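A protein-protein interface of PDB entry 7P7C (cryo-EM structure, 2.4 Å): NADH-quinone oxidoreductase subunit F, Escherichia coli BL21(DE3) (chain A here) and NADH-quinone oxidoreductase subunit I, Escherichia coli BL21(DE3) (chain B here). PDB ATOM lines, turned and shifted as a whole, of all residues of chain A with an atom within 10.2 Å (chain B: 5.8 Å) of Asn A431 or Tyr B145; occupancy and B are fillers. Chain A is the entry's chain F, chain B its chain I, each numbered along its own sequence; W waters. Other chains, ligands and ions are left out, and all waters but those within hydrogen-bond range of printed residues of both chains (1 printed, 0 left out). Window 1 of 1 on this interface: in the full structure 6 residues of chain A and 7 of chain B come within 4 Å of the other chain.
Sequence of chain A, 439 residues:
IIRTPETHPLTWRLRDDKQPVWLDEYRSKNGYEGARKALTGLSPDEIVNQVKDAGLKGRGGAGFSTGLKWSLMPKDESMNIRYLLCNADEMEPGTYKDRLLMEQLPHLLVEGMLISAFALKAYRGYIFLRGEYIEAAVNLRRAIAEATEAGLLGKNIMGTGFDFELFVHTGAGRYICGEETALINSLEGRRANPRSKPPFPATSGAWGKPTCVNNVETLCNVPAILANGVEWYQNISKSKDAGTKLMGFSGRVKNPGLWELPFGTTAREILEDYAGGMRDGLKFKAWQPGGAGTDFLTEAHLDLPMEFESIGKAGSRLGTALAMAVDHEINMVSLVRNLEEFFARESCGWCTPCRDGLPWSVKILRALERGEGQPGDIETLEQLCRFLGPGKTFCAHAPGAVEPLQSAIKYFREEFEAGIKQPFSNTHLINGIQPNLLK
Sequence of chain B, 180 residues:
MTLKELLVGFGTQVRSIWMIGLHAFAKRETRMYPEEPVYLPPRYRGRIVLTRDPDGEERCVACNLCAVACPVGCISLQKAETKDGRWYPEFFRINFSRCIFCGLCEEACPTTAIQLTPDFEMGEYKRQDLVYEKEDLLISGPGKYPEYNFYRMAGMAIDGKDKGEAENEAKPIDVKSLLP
Of the 13 printed residues of chain B, 3 touch a printed residue of chain A.
Hydrophobic or aromatic side chains of chain B that line the printed part of chain A: Tyr B145 and Pro B146.
Hydrophobic or aromatic side chains of chain A that line the printed part of chain B: Ile A433.
Among the printed residues, 5 pairs touch across the chains.
Asn A431 touches Tyr B145.
Pro B146 touches Asn A431 (CG to ND2, 3.4 Å).
Asn A431 touches Glu B147 (ND2 to OE2, 3.8 Å).
O of Gly A432 touches CE1 of Tyr B145, at 3.6 Å.
CE1 of Tyr B145 touches CG1 of Ile A433, 3.6 Å away.
Water W1 lies within hydrogen-bond range of the backbone carbonyl oxygen of Asn A431, the backbone NH of Glu B147 and the backbone NH of Tyr B148.
Of chain B, only Tyr B145 (3.8 Å), Pro B146 (3.4 Å) and Glu B147 (3.8 Å) come within 4 Å of Asn A431.
Tyr B145 touches just these residues of chain A: Asn A431 (3.8 Å), Gly A432 (3.6 Å) and Ile A433 (3.6 Å).
No residue of chain A comes within 4 Å of Thr B112.
No residue of chain A comes within 4 Å of Gly B143.
No residue of chain A comes within 4 Å of Lys B144.
Pro B146 touches just one residue of chain A: Asn A431 (3.4 Å).
Glu B147 touches just one residue of chain A: Asn A431.
Printed residues of chain B within 4 Å of Gly A432: Tyr B145.
Of the printed residues of chain B, Ile A433 touches Tyr B145.
Leu A429 touches none of the printed residues of chain B.
Tyr B148 touches none of the printed residues of chain A.
The nearest residue of chain B that does not touch Asn A431 is Lys B144 (4.3 Å).
The nearest residue of chain A that does not touch Tyr B145 is Ile A430 (5.4 Å).
The guanidinium group (NH2) of Arg B59 is in hydrogen-bond range of the backbone carbonyl oxygen (O) of Tyr B145 (2.9 Å).
The side-chain hydroxyl (OH) of Tyr B145 sits at hydrogen-bond distance from the side-chain carboxylate (OE2) of Glu B106 (3.1 Å).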
ATOM      1  N   HIS A 428      14.413  13.565  -8.760  1.00  0.00           N
ATOM      2  CA  HIS A 428      13.368  12.564  -8.620  1.00  0.00           C
ATOM      3  C   HIS A 428      13.534  11.839  -7.292  1.00  0.00           C
ATOM      4  O   HIS A 428      14.605  11.849  -6.680  1.00  0.00           O
ATOM      5  CB  HIS A 428      13.370  11.569  -9.791  1.00  0.00           C
ATOM      6  CG  HIS A 428      14.682  10.886 -10.025  1.00  0.00           C
ATOM      7  ND1 HIS A 428      15.143   9.860  -9.227  1.00  0.00           N
ATOM      8  CD2 HIS A 428      15.614  11.055 -10.993  1.00  0.00           C
ATOM      9  CE1 HIS A 428      16.312   9.442  -9.681  1.00  0.00           C
ATOM     10  NE2 HIS A 428      16.620  10.151 -10.752  1.00  0.00           N
ATOM     11  N   LEU A 429      12.445  11.232  -6.833  1.00  0.00           N
ATOM     12  CA  LEU A 429      12.469  10.519  -5.565  1.00  0.00           C
ATOM     13  C   LEU A 429      13.207   9.197  -5.720  1.00  0.00           C
ATOM     14  O   LEU A 429      12.959   8.440  -6.663  1.00  0.00           O
ATOM     15  CB  LEU A 429      11.046  10.277  -5.063  1.00  0.00           C
ATOM     16  CG  LEU A 429      10.502  11.246  -4.010  1.00  0.00           C
ATOM     17  CD1 LEU A 429      11.418  11.294  -2.797  1.00  0.00           C
ATOM     18  CD2 LEU A 429      10.306  12.634  -4.591  1.00  0.00           C
ATOM     19  N   ILE A 430      14.119   8.921  -4.795  1.00  0.00           N
ATOM     20  CA  ILE A 430      14.872   7.674  -4.770  1.00  0.00           C
ATOM     21  C   ILE A 430      14.330   6.840  -3.622  1.00  0.00           C
ATOM     22  O   ILE A 430      14.324   7.289  -2.470  1.00  0.00           O
ATOM     23  CB  ILE A 430      16.380   7.923  -4.622  1.00  0.00           C
ATOM     24  CG1 ILE A 430      16.928   8.594  -5.879  1.00  0.00           C
ATOM     25  CG2 ILE A 430      17.114   6.622  -4.354  1.00  0.00           C
ATOM     26  CD1 ILE A 430      18.303   9.164  -5.710  1.00  0.00           C
ATOM     27  N   ASN A 431      13.869   5.634  -3.936  1.00  0.00           N
ATOM     28  CA  ASN A 431      13.225   4.790  -2.941  1.00  0.00           C
ATOM     29  C   ASN A 431      14.242   4.291  -1.923  1.00  0.00           C
ATOM     30  O   ASN A 431      15.241   3.662  -2.281  1.00  0.00           O
ATOM     31  CB  ASN A 431      12.532   3.613  -3.623  1.00  0.00           C
ATOM     32  CG  ASN A 431      11.455   2.996  -2.763  1.00  0.00           C
ATOM     33  OD1 ASN A 431      11.194   3.455  -1.653  1.00  0.00           O
ATOM     34  ND2 ASN A 431      10.820   1.949  -3.272  1.00  0.00           N
ATOM     35  N   GLY A 432      13.979   4.571  -0.649  1.00  0.00           N
ATOM     36  CA  GLY A 432      14.866   4.198   0.429  1.00  0.00           C
ATOM     37  C   GLY A 432      15.676   5.335   1.012  1.00  0.00           C
ATOM     38  O   GLY A 432      16.287   5.153   2.071  1.00  0.00           O
ATOM     39  N   ILE A 433      15.697   6.495   0.365  1.00  0.00           N
ATOM     40  CA  ILE A 433      16.433   7.659   0.847  1.00  0.00           C
ATOM     41  C   ILE A 433      15.436   8.778   1.096  1.00  0.00           C
ATOM     42  O   ILE A 433      14.785   9.255   0.159  1.00  0.00           O
ATOM     43  CB  ILE A 433      17.513   8.109  -0.147  1.00  0.00           C
ATOM     44  CG1 ILE A 433      18.573   7.026  -0.308  1.00  0.00           C
ATOM     45  CG2 ILE A 433      18.157   9.405   0.315  1.00  0.00           C
ATOM     46  CD1 ILE A 433      19.501   7.272  -1.457  1.00  0.00           C
ATOM     47  N   GLN A 434      15.322   9.197   2.345  1.00  0.00           N
ATOM     48  CA  GLN A 434      14.471  10.334   2.674  1.00  0.00           C
ATOM     49  C   GLN A 434      15.161  11.626   2.257  1.00  0.00           C
ATOM     50  O   GLN A 434      16.314  11.854   2.636  1.00  0.00           O
ATOM     51  CB  GLN A 434      14.157  10.360   4.163  1.00  0.00           C
ATOM     52  CG  GLN A 434      13.163   9.301   4.593  1.00  0.00           C
ATOM     53  CD  GLN A 434      13.088   9.148   6.096  1.00  0.00           C
ATOM     54  OE1 GLN A 434      13.948   8.520   6.709  1.00  0.00           O
ATOM     55  NE2 GLN A 434      12.056   9.720   6.698  1.00  0.00           N
ATOM     56  N   PRO A 435      14.507  12.477   1.471  1.00  0.00           N
ATOM     57  CA  PRO A 435      15.156  13.709   1.015  1.00  0.00           C
ATOM     58  C   PRO A 435      15.333  14.717   2.138  1.00  0.00           C
ATOM     59  O   PRO A 435      14.600  14.721   3.129  1.00  0.00           O
ATOM     60  CB  PRO A 435      14.195  14.239  -0.053  1.00  0.00           C
ATOM     61  CG  PRO A 435      12.874  13.680   0.331  1.00  0.00           C
ATOM     62  CD  PRO A 435      13.151  12.327   0.918  1.00  0.00           C
ATOM     63  N   ARG B  52      22.996  -5.556  -6.076  1.00  0.00           N
ATOM     64  CA  ARG B  52      22.894  -5.538  -7.524  1.00  0.00           C
ATOM     65  C   ARG B  52      21.859  -4.510  -7.960  1.00  0.00           C
ATOM     66  O   ARG B  52      20.956  -4.152  -7.204  1.00  0.00           O
ATOM     67  CB  ARG B  52      22.518  -6.920  -8.065  1.00  0.00           C
ATOM     68  CG  ARG B  52      23.565  -7.976  -7.804  1.00  0.00           C
ATOM     69  CD  ARG B  52      23.145  -9.323  -8.338  1.00  0.00           C
ATOM     70  NE  ARG B  52      24.137 -10.345  -8.031  1.00  0.00           N
ATOM     71  CZ  ARG B  52      25.164 -10.650  -8.811  1.00  0.00           C
ATOM     72  NH1 ARG B  52      25.353 -10.047  -9.971  1.00  0.00           N
ATOM     73  NH2 ARG B  52      26.024 -11.581  -8.414  1.00  0.00           N
ATOM     74  N   ARG B  59      26.220  -3.491  -8.467  1.00  0.00           N
ATOM     75  CA  ARG B  59      26.201  -2.037  -8.455  1.00  0.00           C
ATOM     76  C   ARG B  59      27.570  -1.419  -8.221  1.00  0.00           C
ATOM     77  O   ARG B  59      27.747  -0.234  -8.517  1.00  0.00           O
ATOM     78  CB  ARG B  59      25.232  -1.533  -7.387  1.00  0.00           C
ATOM     79  CG  ARG B  59      23.796  -1.585  -7.822  1.00  0.00           C
ATOM     80  CD  ARG B  59      22.935  -0.586  -7.094  1.00  0.00           C
ATOM     81  NE  ARG B  59      22.338  -1.147  -5.892  1.00  0.00           N
ATOM     82  CZ  ARG B  59      21.053  -1.062  -5.587  1.00  0.00           C
ATOM     83  NH1 ARG B  59      20.188  -0.471  -6.393  1.00  0.00           N
ATOM     84  NH2 ARG B  59      20.626  -1.578  -4.442  1.00  0.00           N
ATOM     85  N   GLU B 106      28.769   2.703   3.684  1.00  0.00           N
ATOM     86  CA  GLU B 106      27.466   2.802   3.033  1.00  0.00           C
ATOM     87  C   GLU B 106      27.088   4.255   2.788  1.00  0.00           C
ATOM     88  O   GLU B 106      26.511   4.587   1.748  1.00  0.00           O
ATOM     89  CB  GLU B 106      26.399   2.104   3.875  1.00  0.00           C
ATOM     90  CG  GLU B 106      25.014   2.150   3.260  1.00  0.00           C
ATOM     91  CD  GLU B 106      23.947   1.502   4.117  1.00  0.00           C
ATOM     92  OE1 GLU B 106      24.289   0.780   5.074  1.00  0.00           O
ATOM     93  OE2 GLU B 106      22.757   1.724   3.829  1.00  0.00           O
ATOM     94  N   THR B 112      25.047   3.088  -4.034  1.00  0.00           N
ATOM     95  CA  THR B 112      24.286   2.245  -3.099  1.00  0.00           C
ATOM     96  C   THR B 112      24.617   0.764  -3.266  1.00  0.00           C
ATOM     97  O   THR B 112      23.764  -0.104  -3.078  1.00  0.00           O
ATOM     98  CB  THR B 112      22.771   2.467  -3.202  1.00  0.00           C
ATOM     99  OG1 THR B 112      22.275   1.896  -4.418  1.00  0.00           O
ATOM    100  CG2 THR B 112      22.434   3.940  -3.159  1.00  0.00           C
ATOM    101  N   ILE B 114      27.330  -0.933  -1.526  1.00  0.00           N
ATOM    102  CA  ILE B 114      27.648  -1.482  -0.216  1.00  0.00           C
ATOM    103  C   ILE B 114      26.572  -1.050   0.773  1.00  0.00           C
ATOM    104  O   ILE B 114      26.167   0.118   0.809  1.00  0.00           O
ATOM    105  CB  ILE B 114      29.067  -1.063   0.217  1.00  0.00           C
ATOM    106  CG1 ILE B 114      29.471  -1.723   1.521  1.00  0.00           C
ATOM    107  CG2 ILE B 114      29.239   0.436   0.327  1.00  0.00           C
ATOM    108  CD1 ILE B 114      30.964  -1.766   1.728  1.00  0.00           C
ATOM    109  N   GLN B 115      26.038  -2.013   1.517  1.00  0.00           N
ATOM    110  CA  GLN B 115      24.949  -1.747   2.443  1.00  0.00           C
ATOM    111  C   GLN B 115      25.170  -2.527   3.727  1.00  0.00           C
ATOM    112  O   GLN B 115      25.693  -3.641   3.712  1.00  0.00           O
ATOM    113  CB  GLN B 115      23.583  -2.123   1.853  1.00  0.00           C
ATOM    114  CG  GLN B 115      23.141  -1.279   0.673  1.00  0.00           C
ATOM    115  CD  GLN B 115      21.906  -1.825   0.000  1.00  0.00           C
ATOM    116  OE1 GLN B 115      21.155  -2.595   0.591  1.00  0.00           O
ATOM    117  NE2 GLN B 115      21.697  -1.443  -1.251  1.00  0.00           N
ATOM    118  N   PRO B 142      18.698  -5.991  -4.895  1.00  0.00           N
ATOM    119  CA  PRO B 142      19.050  -4.590  -4.629  1.00  0.00           C
ATOM    120  C   PRO B 142      19.165  -4.218  -3.160  1.00  0.00           C
ATOM    121  O   PRO B 142      19.686  -3.137  -2.863  1.00  0.00           O
ATOM    122  CB  PRO B 142      17.910  -3.820  -5.296  1.00  0.00           C
ATOM    123  CG  PRO B 142      16.758  -4.739  -5.219  1.00  0.00           C
ATOM    124  CD  PRO B 142      17.306  -6.129  -5.356  1.00  0.00           C
ATOM    125  N   GLY B 143      18.703  -5.055  -2.241  1.00  0.00           N
ATOM    126  CA  GLY B 143      18.840  -4.724  -0.831  1.00  0.00           C
ATOM    127  C   GLY B 143      17.876  -3.628  -0.417  1.00  0.00           C
ATOM    128  O   GLY B 143      16.691  -3.647  -0.764  1.00  0.00           O
ATOM    129  N   LYS B 144      18.390  -2.653   0.332  1.00  0.00           N
ATOM    130  CA  LYS B 144      17.552  -1.614   0.917  1.00  0.00           C
ATOM    131  C   LYS B 144      17.155  -0.532  -0.076  1.00  0.00           C
ATOM    132  O   LYS B 144      16.248   0.250   0.217  1.00  0.00           O
ATOM    133  CB  LYS B 144      18.266  -0.970   2.106  1.00  0.00           C
ATOM    134  CG  LYS B 144      18.657  -1.947   3.194  1.00  0.00           C
ATOM    135  CD  LYS B 144      19.094  -1.229   4.454  1.00  0.00           C
ATOM    136  CE  LYS B 144      20.427  -0.543   4.260  1.00  0.00           C
ATOM    137  NZ  LYS B 144      21.043  -0.164   5.555  1.00  0.00           N
ATOM    138  N   TYR B 145      17.814  -0.455  -1.227  1.00  0.00           N
ATOM    139  CA  TYR B 145      17.498   0.544  -2.248  1.00  0.00           C
ATOM    140  C   TYR B 145      17.072  -0.185  -3.511  1.00  0.00           C
ATOM    141  O   TYR B 145      17.928  -0.649  -4.285  1.00  0.00           O
ATOM    142  CB  TYR B 145      18.697   1.454  -2.508  1.00  0.00           C
ATOM    143  CG  TYR B 145      19.275   2.029  -1.235  1.00  0.00           C
ATOM    144  CD1 TYR B 145      18.671   3.103  -0.601  1.00  0.00           C
ATOM    145  CD2 TYR B 145      20.407   1.481  -0.654  1.00  0.00           C
ATOM    146  CE1 TYR B 145      19.184   3.620   0.566  1.00  0.00           C
ATOM    147  CE2 TYR B 145      20.930   1.991   0.512  1.00  0.00           C
ATOM    148  CZ  TYR B 145      20.315   3.062   1.117  1.00  0.00           C
ATOM    149  OH  TYR B 145      20.830   3.578   2.282  1.00  0.00           O
ATOM    150  N   PRO B 146      15.768  -0.321  -3.765  1.00  0.00           N
ATOM    151  CA  PRO B 146      15.305  -1.265  -4.789  1.00  0.00           C
ATOM    152  C   PRO B 146      15.416  -0.784  -6.226  1.00  0.00           C
ATOM    153  O   PRO B 146      15.263  -1.608  -7.136  1.00  0.00           O
ATOM    154  CB  PRO B 146      13.837  -1.487  -4.408  1.00  0.00           C
ATOM    155  CG  PRO B 146      13.440  -0.238  -3.725  1.00  0.00           C
ATOM    156  CD  PRO B 146      14.652   0.268  -3.005  1.00  0.00           C
ATOM    157  N   GLU B 147      15.673   0.499  -6.479  1.00  0.00           N
ATOM    158  CA  GLU B 147      15.549   1.021  -7.832  1.00  0.00           C
ATOM    159  C   GLU B 147      16.751   1.788  -8.357  1.00  0.00           C
ATOM    160  O   GLU B 147      16.848   1.955  -9.576  1.00  0.00           O
ATOM    161  CB  GLU B 147      14.318   1.935  -7.938  1.00  0.00           C
ATOM    162  CG  GLU B 147      13.133   1.303  -8.637  1.00  0.00           C
ATOM    163  CD  GLU B 147      12.355   0.374  -7.733  1.00  0.00           C
ATOM    164  OE1 GLU B 147      12.325  -0.842  -8.013  1.00  0.00           O
ATOM    165  OE2 GLU B 147      11.771   0.859  -6.740  1.00  0.00           O
ATOM    166  N   TYR B 148      17.654   2.265  -7.503  1.00  0.00           N
ATOM    167  CA  TYR B 148      18.709   3.155  -7.969  1.00  0.00           C
ATOM    168  C   TYR B 148      19.725   2.414  -8.827  1.00  0.00           C
ATOM    169  O   TYR B 148      20.125   1.289  -8.524  1.00  0.00           O
ATOM    170  CB  TYR B 148      19.421   3.825  -6.796  1.00  0.00           C
ATOM    171  CG  TYR B 148      20.451   4.825  -7.259  1.00  0.00           C
ATOM    172  CD1 TYR B 148      20.065   6.039  -7.805  1.00  0.00           C
ATOM    173  CD2 TYR B 148      21.809   4.541  -7.182  1.00  0.00           C
ATOM    174  CE1 TYR B 148      20.997   6.948  -8.244  1.00  0.00           C
ATOM    175  CE2 TYR B 148      22.746   5.446  -7.619  1.00  0.00           C
ATOM    176  CZ  TYR B 148      22.337   6.648  -8.148  1.00  0.00           C
ATOM    177  OH  TYR B 148      23.268   7.554  -8.585  1.00  0.00           O
HETATM  178  O   HOH W   1      16.090   3.157  -4.885  1.00  0.00           O
